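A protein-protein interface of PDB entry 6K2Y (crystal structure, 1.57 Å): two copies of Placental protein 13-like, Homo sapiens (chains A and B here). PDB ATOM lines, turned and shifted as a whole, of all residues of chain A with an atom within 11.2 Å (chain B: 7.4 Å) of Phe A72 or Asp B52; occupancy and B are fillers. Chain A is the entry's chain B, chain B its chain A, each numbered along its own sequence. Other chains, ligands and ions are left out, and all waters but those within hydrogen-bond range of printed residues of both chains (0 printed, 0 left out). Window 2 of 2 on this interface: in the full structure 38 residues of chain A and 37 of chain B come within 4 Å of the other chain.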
ATOM      1  N   ASN A  68      16.560  18.577  -6.661  1.00  0.00           N
ATOM      2  CA  ASN A  68      15.652  19.595  -7.176  1.00  0.00           C
ATOM      3  C   ASN A  68      16.099  20.956  -6.658  1.00  0.00           C
ATOM      4  O   ASN A  68      17.059  21.070  -5.893  1.00  0.00           O
ATOM      5  CB  ASN A  68      14.215  19.297  -6.756  1.00  0.00           C
ATOM      6  CG  ASN A  68      13.176  19.784  -7.779  1.00  0.00           C
ATOM      7  OD1 ASN A  68      12.025  19.339  -7.752  1.00  0.00           O
ATOM      8  ND2 ASN A  68      13.576  20.688  -8.666  1.00  0.00           N
ATOM      9  N   SER A  69      15.380  21.991  -7.089  1.00  0.00           N
ATOM     10  CA  SER A  69      15.535  23.343  -6.579  1.00  0.00           C
ATOM     11  C   SER A  69      14.151  23.879  -6.247  1.00  0.00           C
ATOM     12  O   SER A  69      13.136  23.400  -6.758  1.00  0.00           O
ATOM     13  CB  SER A  69      16.240  24.259  -7.596  1.00  0.00           C
ATOM     14  OG  SER A  69      15.547  24.275  -8.851  1.00  0.00           O
ATOM     15  N   CYS A  70      14.118  24.855  -5.347  1.00  0.00           N
ATOM     16  CA  CYS A  70      12.883  25.529  -4.969  1.00  0.00           C
ATOM     17  C   CYS A  70      13.080  27.008  -5.236  1.00  0.00           C
ATOM     18  O   CYS A  70      13.944  27.636  -4.621  1.00  0.00           O
ATOM     19  CB  CYS A  70      12.523  25.286  -3.510  1.00  0.00           C
ATOM     20  SG  CYS A  70      10.854  25.925  -3.127  1.00  0.00           S
ATOM     21  N   VAL A  71      12.321  27.549  -6.187  1.00  0.00           N
ATOM     22  CA  VAL A  71      12.500  28.920  -6.641  1.00  0.00           C
ATOM     23  C   VAL A  71      11.142  29.603  -6.566  1.00  0.00           C
ATOM     24  O   VAL A  71      10.154  29.063  -7.067  1.00  0.00           O
ATOM     25  CB  VAL A  71      13.069  28.972  -8.074  1.00  0.00           C
ATOM     26  CG1 VAL A  71      13.429  30.405  -8.470  1.00  0.00           C
ATOM     27  CG2 VAL A  71      14.292  28.052  -8.194  1.00  0.00           C
ATOM     28  N   PHE A  72      11.088  30.760  -5.895  1.00  0.00           N
ATOM     29  CA  PHE A  72       9.828  31.478  -5.659  1.00  0.00           C
ATOM     30  C   PHE A  72       8.799  30.610  -4.930  1.00  0.00           C
ATOM     31  O   PHE A  72       7.593  30.722  -5.166  1.00  0.00           O
ATOM     32  CB  PHE A  72       9.254  32.018  -6.974  1.00  0.00           C
ATOM     33  CG  PHE A  72      10.219  32.870  -7.747  1.00  0.00           C
ATOM     34  CD1 PHE A  72      10.929  33.884  -7.119  1.00  0.00           C
ATOM     35  CD2 PHE A  72      10.435  32.645  -9.090  1.00  0.00           C
ATOM     36  CE1 PHE A  72      11.826  34.675  -7.829  1.00  0.00           C
ATOM     37  CE2 PHE A  72      11.334  33.422  -9.810  1.00  0.00           C
ATOM     38  CZ  PHE A  72      12.034  34.439  -9.176  1.00  0.00           C
ATOM     39  N   GLY A  73       9.262  29.743  -4.030  1.00  0.00           N
ATOM     40  CA  GLY A  73       8.399  28.840  -3.295  1.00  0.00           C
ATOM     41  C   GLY A  73       7.933  27.618  -4.052  1.00  0.00           C
ATOM     42  O   GLY A  73       7.165  26.823  -3.495  1.00  0.00           O
ATOM     43  N   ILE A  74       8.384  27.428  -5.286  1.00  0.00           N
ATOM     44  CA  ILE A  74       7.904  26.375  -6.174  1.00  0.00           C
ATOM     45  C   ILE A  74       9.041  25.390  -6.413  1.00  0.00           C
ATOM     46  O   ILE A  74      10.103  25.775  -6.919  1.00  0.00           O
ATOM     47  CB  ILE A  74       7.412  26.960  -7.509  1.00  0.00           C
ATOM     48  CG1 ILE A  74       6.181  27.838  -7.294  1.00  0.00           C
ATOM     49  CG2 ILE A  74       7.131  25.865  -8.522  1.00  0.00           C
ATOM     50  CD1 ILE A  74       5.210  27.306  -6.266  1.00  0.00           C
ATOM     51  N   TRP A  75       8.822  24.119  -6.070  1.00  0.00           N
ATOM     52  CA  TRP A  75       9.754  23.079  -6.484  1.00  0.00           C
ATOM     53  C   TRP A  75       9.701  22.920  -7.996  1.00  0.00           C
ATOM     54  O   TRP A  75       8.632  23.018  -8.609  1.00  0.00           O
ATOM     55  CB  TRP A  75       9.427  21.749  -5.793  1.00  0.00           C
ATOM     56  CG  TRP A  75       9.825  21.727  -4.360  1.00  0.00           C
ATOM     57  CD1 TRP A  75       9.001  21.758  -3.281  1.00  0.00           C
ATOM     58  CD2 TRP A  75      11.162  21.680  -3.844  1.00  0.00           C
ATOM     59  NE1 TRP A  75       9.735  21.745  -2.119  1.00  0.00           N
ATOM     60  CE2 TRP A  75      11.066  21.687  -2.439  1.00  0.00           C
ATOM     61  CE3 TRP A  75      12.430  21.623  -4.437  1.00  0.00           C
ATOM     62  CZ2 TRP A  75      12.189  21.646  -1.613  1.00  0.00           C
ATOM     63  CZ3 TRP A  75      13.547  21.586  -3.616  1.00  0.00           C
ATOM     64  CH2 TRP A  75      13.417  21.596  -2.223  1.00  0.00           C
ATOM     65  N   ARG A  76      10.861  22.681  -8.604  1.00  0.00           N
ATOM     66  CA  ARG A  76      11.010  22.702 -10.046  1.00  0.00           C
ATOM     67  C   ARG A  76      11.146  21.263 -10.562  1.00  0.00           C
ATOM     68  O   ARG A  76      10.523  20.347 -10.002  1.00  0.00           O
ATOM     69  CB  ARG A  76      12.172  23.621 -10.409  1.00  0.00           C
ATOM     70  CG  ARG A  76      11.978  25.084  -9.946  1.00  0.00           C
ATOM     71  CD  ARG A  76      10.567  25.618 -10.301  1.00  0.00           C
ATOM     72  NE  ARG A  76      10.287  26.938  -9.726  1.00  0.00           N
ATOM     73  CZ  ARG A  76       9.903  28.007 -10.427  1.00  0.00           C
ATOM     74  NH1 ARG A  76       9.752  27.932 -11.743  1.00  0.00           N
ATOM     75  NH2 ARG A  76       9.656  29.151  -9.805  1.00  0.00           N
ATOM     76  N   ASN B  42      19.751  20.433   2.085  1.00  0.00           N
ATOM     77  CA  ASN B  42      19.292  21.609   1.343  1.00  0.00           C
ATOM     78  C   ASN B  42      20.366  22.690   1.343  1.00  0.00           C
ATOM     79  O   ASN B  42      20.963  22.976   2.385  1.00  0.00           O
ATOM     80  CB  ASN B  42      18.006  22.177   1.949  1.00  0.00           C
ATOM     81  CG  ASN B  42      16.839  21.242   1.793  1.00  0.00           C
ATOM     82  OD1 ASN B  42      16.602  20.697   0.723  1.00  0.00           O
ATOM     83  ND2 ASN B  42      16.111  21.026   2.876  1.00  0.00           N
ATOM     84  N   PHE B  43      20.604  23.285   0.168  1.00  0.00           N
ATOM     85  CA  PHE B  43      21.444  24.475   0.018  1.00  0.00           C
ATOM     86  C   PHE B  43      20.496  25.654  -0.182  1.00  0.00           C
ATOM     87  O   PHE B  43      19.842  25.751  -1.225  1.00  0.00           O
ATOM     88  CB  PHE B  43      22.384  24.400  -1.192  1.00  0.00           C
ATOM     89  CG  PHE B  43      23.472  23.362  -1.119  1.00  0.00           C
ATOM     90  CD1 PHE B  43      23.631  22.513  -0.036  1.00  0.00           C
ATOM     91  CD2 PHE B  43      24.349  23.251  -2.186  1.00  0.00           C
ATOM     92  CE1 PHE B  43      24.652  21.561  -0.025  1.00  0.00           C
ATOM     93  CE2 PHE B  43      25.371  22.316  -2.183  1.00  0.00           C
ATOM     94  CZ  PHE B  43      25.515  21.465  -1.124  1.00  0.00           C
ATOM     95  N   TYR B  44      20.424  26.543   0.798  1.00  0.00           N
ATOM     96  CA  TYR B  44      19.531  27.693   0.715  1.00  0.00           C
ATOM     97  C   TYR B  44      20.286  28.919   0.220  1.00  0.00           C
ATOM     98  O   TYR B  44      21.486  29.076   0.467  1.00  0.00           O
ATOM     99  CB  TYR B  44      18.902  28.013   2.074  1.00  0.00           C
ATOM    100  CG  TYR B  44      17.882  27.037   2.586  1.00  0.00           C
ATOM    101  CD1 TYR B  44      18.270  25.905   3.295  1.00  0.00           C
ATOM    102  CD2 TYR B  44      16.519  27.270   2.411  1.00  0.00           C
ATOM    103  CE1 TYR B  44      17.322  25.017   3.794  1.00  0.00           C
ATOM    104  CE2 TYR B  44      15.572  26.381   2.905  1.00  0.00           C
ATOM    105  CZ  TYR B  44      15.980  25.260   3.590  1.00  0.00           C
ATOM    106  OH  TYR B  44      15.033  24.383   4.085  1.00  0.00           O
ATOM    107  N   THR B  45      19.559  29.813  -0.456  1.00  0.00           N
ATOM    108  CA  THR B  45      20.119  31.068  -0.946  1.00  0.00           C
ATOM    109  C   THR B  45      19.926  32.223   0.038  1.00  0.00           C
ATOM    110  O   THR B  45      20.205  33.376  -0.308  1.00  0.00           O
ATOM    111  CB  THR B  45      19.499  31.425  -2.302  1.00  0.00           C
ATOM    112  OG1 THR B  45      18.097  31.639  -2.129  1.00  0.00           O
ATOM    113  CG2 THR B  45      19.703  30.287  -3.299  1.00  0.00           C
ATOM    114  N   GLY B  46      19.450  31.936   1.246  1.00  0.00           N
ATOM    115  CA  GLY B  46      19.311  32.930   2.293  1.00  0.00           C
ATOM    116  C   GLY B  46      19.298  32.205   3.619  1.00  0.00           C
ATOM    117  O   GLY B  46      19.470  30.986   3.679  1.00  0.00           O
ATOM    118  N   ASP B  48      16.682  32.437   5.942  1.00  0.00           N
ATOM    119  CA  ASP B  48      15.351  32.095   6.423  1.00  0.00           C
ATOM    120  C   ASP B  48      14.925  30.738   5.877  1.00  0.00           C
ATOM    121  O   ASP B  48      15.430  30.268   4.856  1.00  0.00           O
ATOM    122  CB  ASP B  48      14.329  33.153   6.009  1.00  0.00           C
ATOM    123  CG  ASP B  48      14.820  34.562   6.246  1.00  0.00           C
ATOM    124  OD1 ASP B  48      15.618  34.769   7.186  1.00  0.00           O
ATOM    125  OD2 ASP B  48      14.402  35.465   5.491  1.00  0.00           O
ATOM    126  N   GLU B  49      13.979  30.105   6.574  1.00  0.00           N
ATOM    127  CA  GLU B  49      13.302  28.961   5.976  1.00  0.00           C
ATOM    128  C   GLU B  49      12.451  29.382   4.791  1.00  0.00           C
ATOM    129  O   GLU B  49      12.016  28.525   4.015  1.00  0.00           O
ATOM    130  CB  GLU B  49      12.435  28.246   7.016  1.00  0.00           C
ATOM    131  CG  GLU B  49      12.267  26.745   6.771  1.00  0.00           C
ATOM    132  CD  GLU B  49      13.502  25.926   7.144  1.00  0.00           C
ATOM    133  OE1 GLU B  49      13.411  24.678   7.123  1.00  0.00           O
ATOM    134  OE2 GLU B  49      14.554  26.521   7.469  1.00  0.00           O
ATOM    135  N   ASP B  50      12.225  30.689   4.648  1.00  0.00           N
ATOM    136  CA  ASP B  50      11.491  31.271   3.539  1.00  0.00           C
ATOM    137  C   ASP B  50      12.281  31.261   2.240  1.00  0.00           C
ATOM    138  O   ASP B  50      11.677  31.338   1.168  1.00  0.00           O
ATOM    139  CB  ASP B  50      11.125  32.715   3.897  1.00  0.00           C
ATOM    140  CG  ASP B  50       9.746  33.107   3.426  1.00  0.00           C
ATOM    141  OD1 ASP B  50       9.030  32.238   2.882  1.00  0.00           O
ATOM    142  OD2 ASP B  50       9.382  34.291   3.610  1.00  0.00           O
ATOM    143  N   SER B  51      13.611  31.193   2.301  1.00  0.00           N
ATOM    144  CA  SER B  51      14.401  31.496   1.120  1.00  0.00           C
ATOM    145  C   SER B  51      14.383  30.329   0.133  1.00  0.00           C
ATOM    146  O   SER B  51      13.935  29.223   0.441  1.00  0.00           O
ATOM    147  CB  SER B  51      15.838  31.853   1.503  1.00  0.00           C
ATOM    148  OG  SER B  51      16.351  30.946   2.452  1.00  0.00           O
ATOM    149  N   ASP B  52      14.879  30.606  -1.068  1.00  0.00           N
ATOM    150  CA  ASP B  52      14.930  29.614  -2.128  1.00  0.00           C
ATOM    151  C   ASP B  52      15.958  28.534  -1.804  1.00  0.00           C
ATOM    152  O   ASP B  52      16.864  28.723  -0.993  1.00  0.00           O
ATOM    153  CB  ASP B  52      15.285  30.263  -3.464  1.00  0.00           C
ATOM    154  CG  ASP B  52      14.185  31.182  -3.988  1.00  0.00           C
ATOM    155  OD1 ASP B  52      12.993  30.923  -3.713  1.00  0.00           O
ATOM    156  OD2 ASP B  52      14.532  32.169  -4.664  1.00  0.00           O
ATOM    157  N   ILE B  53      15.803  27.392  -2.457  1.00  0.00           N
ATOM    158  CA  ILE B  53      16.732  26.271  -2.319  1.00  0.00           C
ATOM    159  C   ILE B  53      17.418  26.077  -3.663  1.00  0.00           C
ATOM    160  O   ILE B  53      16.781  25.683  -4.651  1.00  0.00           O
ATOM    161  CB  ILE B  53      16.028  24.995  -1.841  1.00  0.00           C
ATOM    162  CG1 ILE B  53      15.531  25.216  -0.410  1.00  0.00           C
ATOM    163  CG2 ILE B  53      16.964  23.789  -1.928  1.00  0.00           C
ATOM    164  CD1 ILE B  53      14.633  24.108   0.162  1.00  0.00           C
ATOM    165  N   ALA B  54      18.720  26.369  -3.700  1.00  0.00           N
ATOM    166  CA  ALA B  54      19.488  26.193  -4.922  1.00  0.00           C
ATOM    167  C   ALA B  54      19.645  24.728  -5.275  1.00  0.00           C
ATOM    168  O   ALA B  54      19.771  24.386  -6.457  1.00  0.00           O
ATOM    169  CB  ALA B  54      20.865  26.833  -4.772  1.00  0.00           C
ATOM    170  N   PHE B  55      19.676  23.856  -4.270  1.00  0.00           N
ATOM    171  CA  PHE B  55      19.985  22.450  -4.503  1.00  0.00           C
ATOM    172  C   PHE B  55      19.480  21.672  -3.305  1.00  0.00           C
ATOM    173  O   PHE B  55      19.847  21.980  -2.166  1.00  0.00           O
ATOM    174  CB  PHE B  55      21.501  22.247  -4.709  1.00  0.00           C
ATOM    175  CG  PHE B  55      21.926  20.806  -4.782  1.00  0.00           C
ATOM    176  CD1 PHE B  55      21.657  20.047  -5.910  1.00  0.00           C
ATOM    177  CD2 PHE B  55      22.595  20.209  -3.722  1.00  0.00           C
ATOM    178  CE1 PHE B  55      22.064  18.714  -5.991  1.00  0.00           C
ATOM    179  CE2 PHE B  55      23.001  18.872  -3.788  1.00  0.00           C
ATOM    180  CZ  PHE B  55      22.747  18.130  -4.933  1.00  0.00           C
ATOM    181  N   PHE B 119      21.388  28.167  -9.736  1.00  0.00           N
ATOM    182  CA  PHE B 119      21.843  29.437  -9.198  1.00  0.00           C
ATOM    183  C   PHE B 119      23.360  29.458  -9.282  1.00  0.00           C
ATOM    184  O   PHE B 119      23.997  28.400  -9.235  1.00  0.00           O
ATOM    185  CB  PHE B 119      21.455  29.624  -7.724  1.00  0.00           C
ATOM    186  CG  PHE B 119      19.980  29.789  -7.466  1.00  0.00           C
ATOM    187  CD1 PHE B 119      19.134  28.695  -7.460  1.00  0.00           C
ATOM    188  CD2 PHE B 119      19.453  31.039  -7.169  1.00  0.00           C
ATOM    189  CE1 PHE B 119      17.784  28.839  -7.186  1.00  0.00           C
ATOM    190  CE2 PHE B 119      18.111  31.198  -6.904  1.00  0.00           C
ATOM    191  CZ  PHE B 119      17.267  30.095  -6.910  1.00  0.00           C
ATOM    192  N   SER B 123      25.520  32.036  -4.622  1.00  0.00           N
ATOM    193  CA  SER B 123      24.220  32.378  -4.061  1.00  0.00           C
ATOM    194  C   SER B 123      23.908  31.583  -2.807  1.00  0.00           C
ATOM    195  O   SER B 123      23.013  31.979  -2.054  1.00  0.00           O
ATOM    196  CB  SER B 123      23.101  32.137  -5.075  1.00  0.00           C
ATOM    197  OG  SER B 123      23.077  33.150  -6.064  1.00  0.00           O
ATOM    198  N   MET B 126      23.419  28.958   3.166  1.00  0.00           N
ATOM    199  CA  MET B 126      23.069  28.180   4.344  1.00  0.00           C
ATOM    200  C   MET B 126      22.856  26.733   3.932  1.00  0.00           C
ATOM    201  O   MET B 126      22.290  26.458   2.873  1.00  0.00           O
ATOM    202  CB  MET B 126      21.798  28.722   5.017  1.00  0.00           C
ATOM    203  CG  MET B 126      21.350  27.979   6.268  1.00  0.00           C
ATOM    204  SD  MET B 126      19.899  28.779   7.019  1.00  0.00           S
ATOM    205  CE  MET B 126      18.597  28.291   5.895  1.00  0.00           C
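N of Phe A72 lies within hydrogen-bond range of OD1 of Asp B52 (2.9 Å).
The backbone carbonyl oxygen of Cys A70 is in hydrogen-bond range of the backbone NH of Ile B53.
N of Ile A74 is in hydrogen-bond range of SG of Cys A70 (3.6 Å).
OD1 of Asn A68 lies close to O of Arg A76.
The guanidinium group (NH2) of Arg A76 is in hydrogen-bond range of the backbone carbonyl oxygen (O) of Val A71, at 2.8 Å.
The backbone NH (N) of Arg A76 lies within hydrogen-bond range of the backbone carbonyl oxygen (O) of Ser A69.
N of Thr B45 lies within hydrogen-bond range of O of Asp B52 (3.0 Å).
The backbone carbonyl oxygen of Phe B55 is in hydrogen-bond range of the backbone NH of Phe B43, 2.8 Å away.
Of the 9 printed residues of chain A, 7 touch a printed residue of chain B.
Hydrophobic or aromatic side chains of chain A that line the printed part of chain B: Val A71 and Trp A75.
Hydrophobic or aromatic side chains of chain B within 4 Å of the printed part of chain A: Ile B53 and Phe B119.
Among the printed residues, 10 pairs touch across the chains.
Phe B55 touches Asn A68.
O of Ile B53 touches CA of Ser A69, 3.3 Å away.
CB of Ser A69 touches O of Ala B54, at 3.7 Å.
Asp B52 touches Cys A70.
Val A71 touches Asp B52.
CE1 of Phe B119 touches CG2 of Val A71 (3.7 Å).
Asp B52 touches Gly A73.
CD1 of Ile B53 touches CH2 of Trp A75, at 3.7 Å.
Of chain B, only Asp B52 (2.9 Å) comes within 4 Å of Phe A72.
Asp B52 touches just these residues of chain A: Cys A70 (3.2 Å), Val A71 (3.6 Å), Phe A72 (2.9 Å) and Gly A73 (3.9 Å).
No residue of chain A comes within 4 Å of Tyr B44.
No residue of chain A comes within 4 Å of Thr B45.
No residue of chain A comes within 4 Å of Gly B46.
No residue of chain A comes within 4 Å of Ser B51.
Of the printed residues of chain B, Val A71 touches Asp B52 (3.6 Å) and Phe B119 (3.7 Å).
Of the printed residues of chain B, Gly A73 touches Asp B52 (3.9 Å).
Of the printed residues of chain B, Ser A69 touches Ile B53 (3.3 Å) and Ala B54 (3.7 Å).
Arg A76 touches none of the printed residues of chain B.
Asp B48 touches none of the printed residues of chain A.
The nearest residue of chain B that does not touch Phe A72 is Phe B119 (6.3 Å).
The nearest printed residue of chain B that does not touch Ser A69 is Phe B55 (4.8 Å).
No position is printed for both chains.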
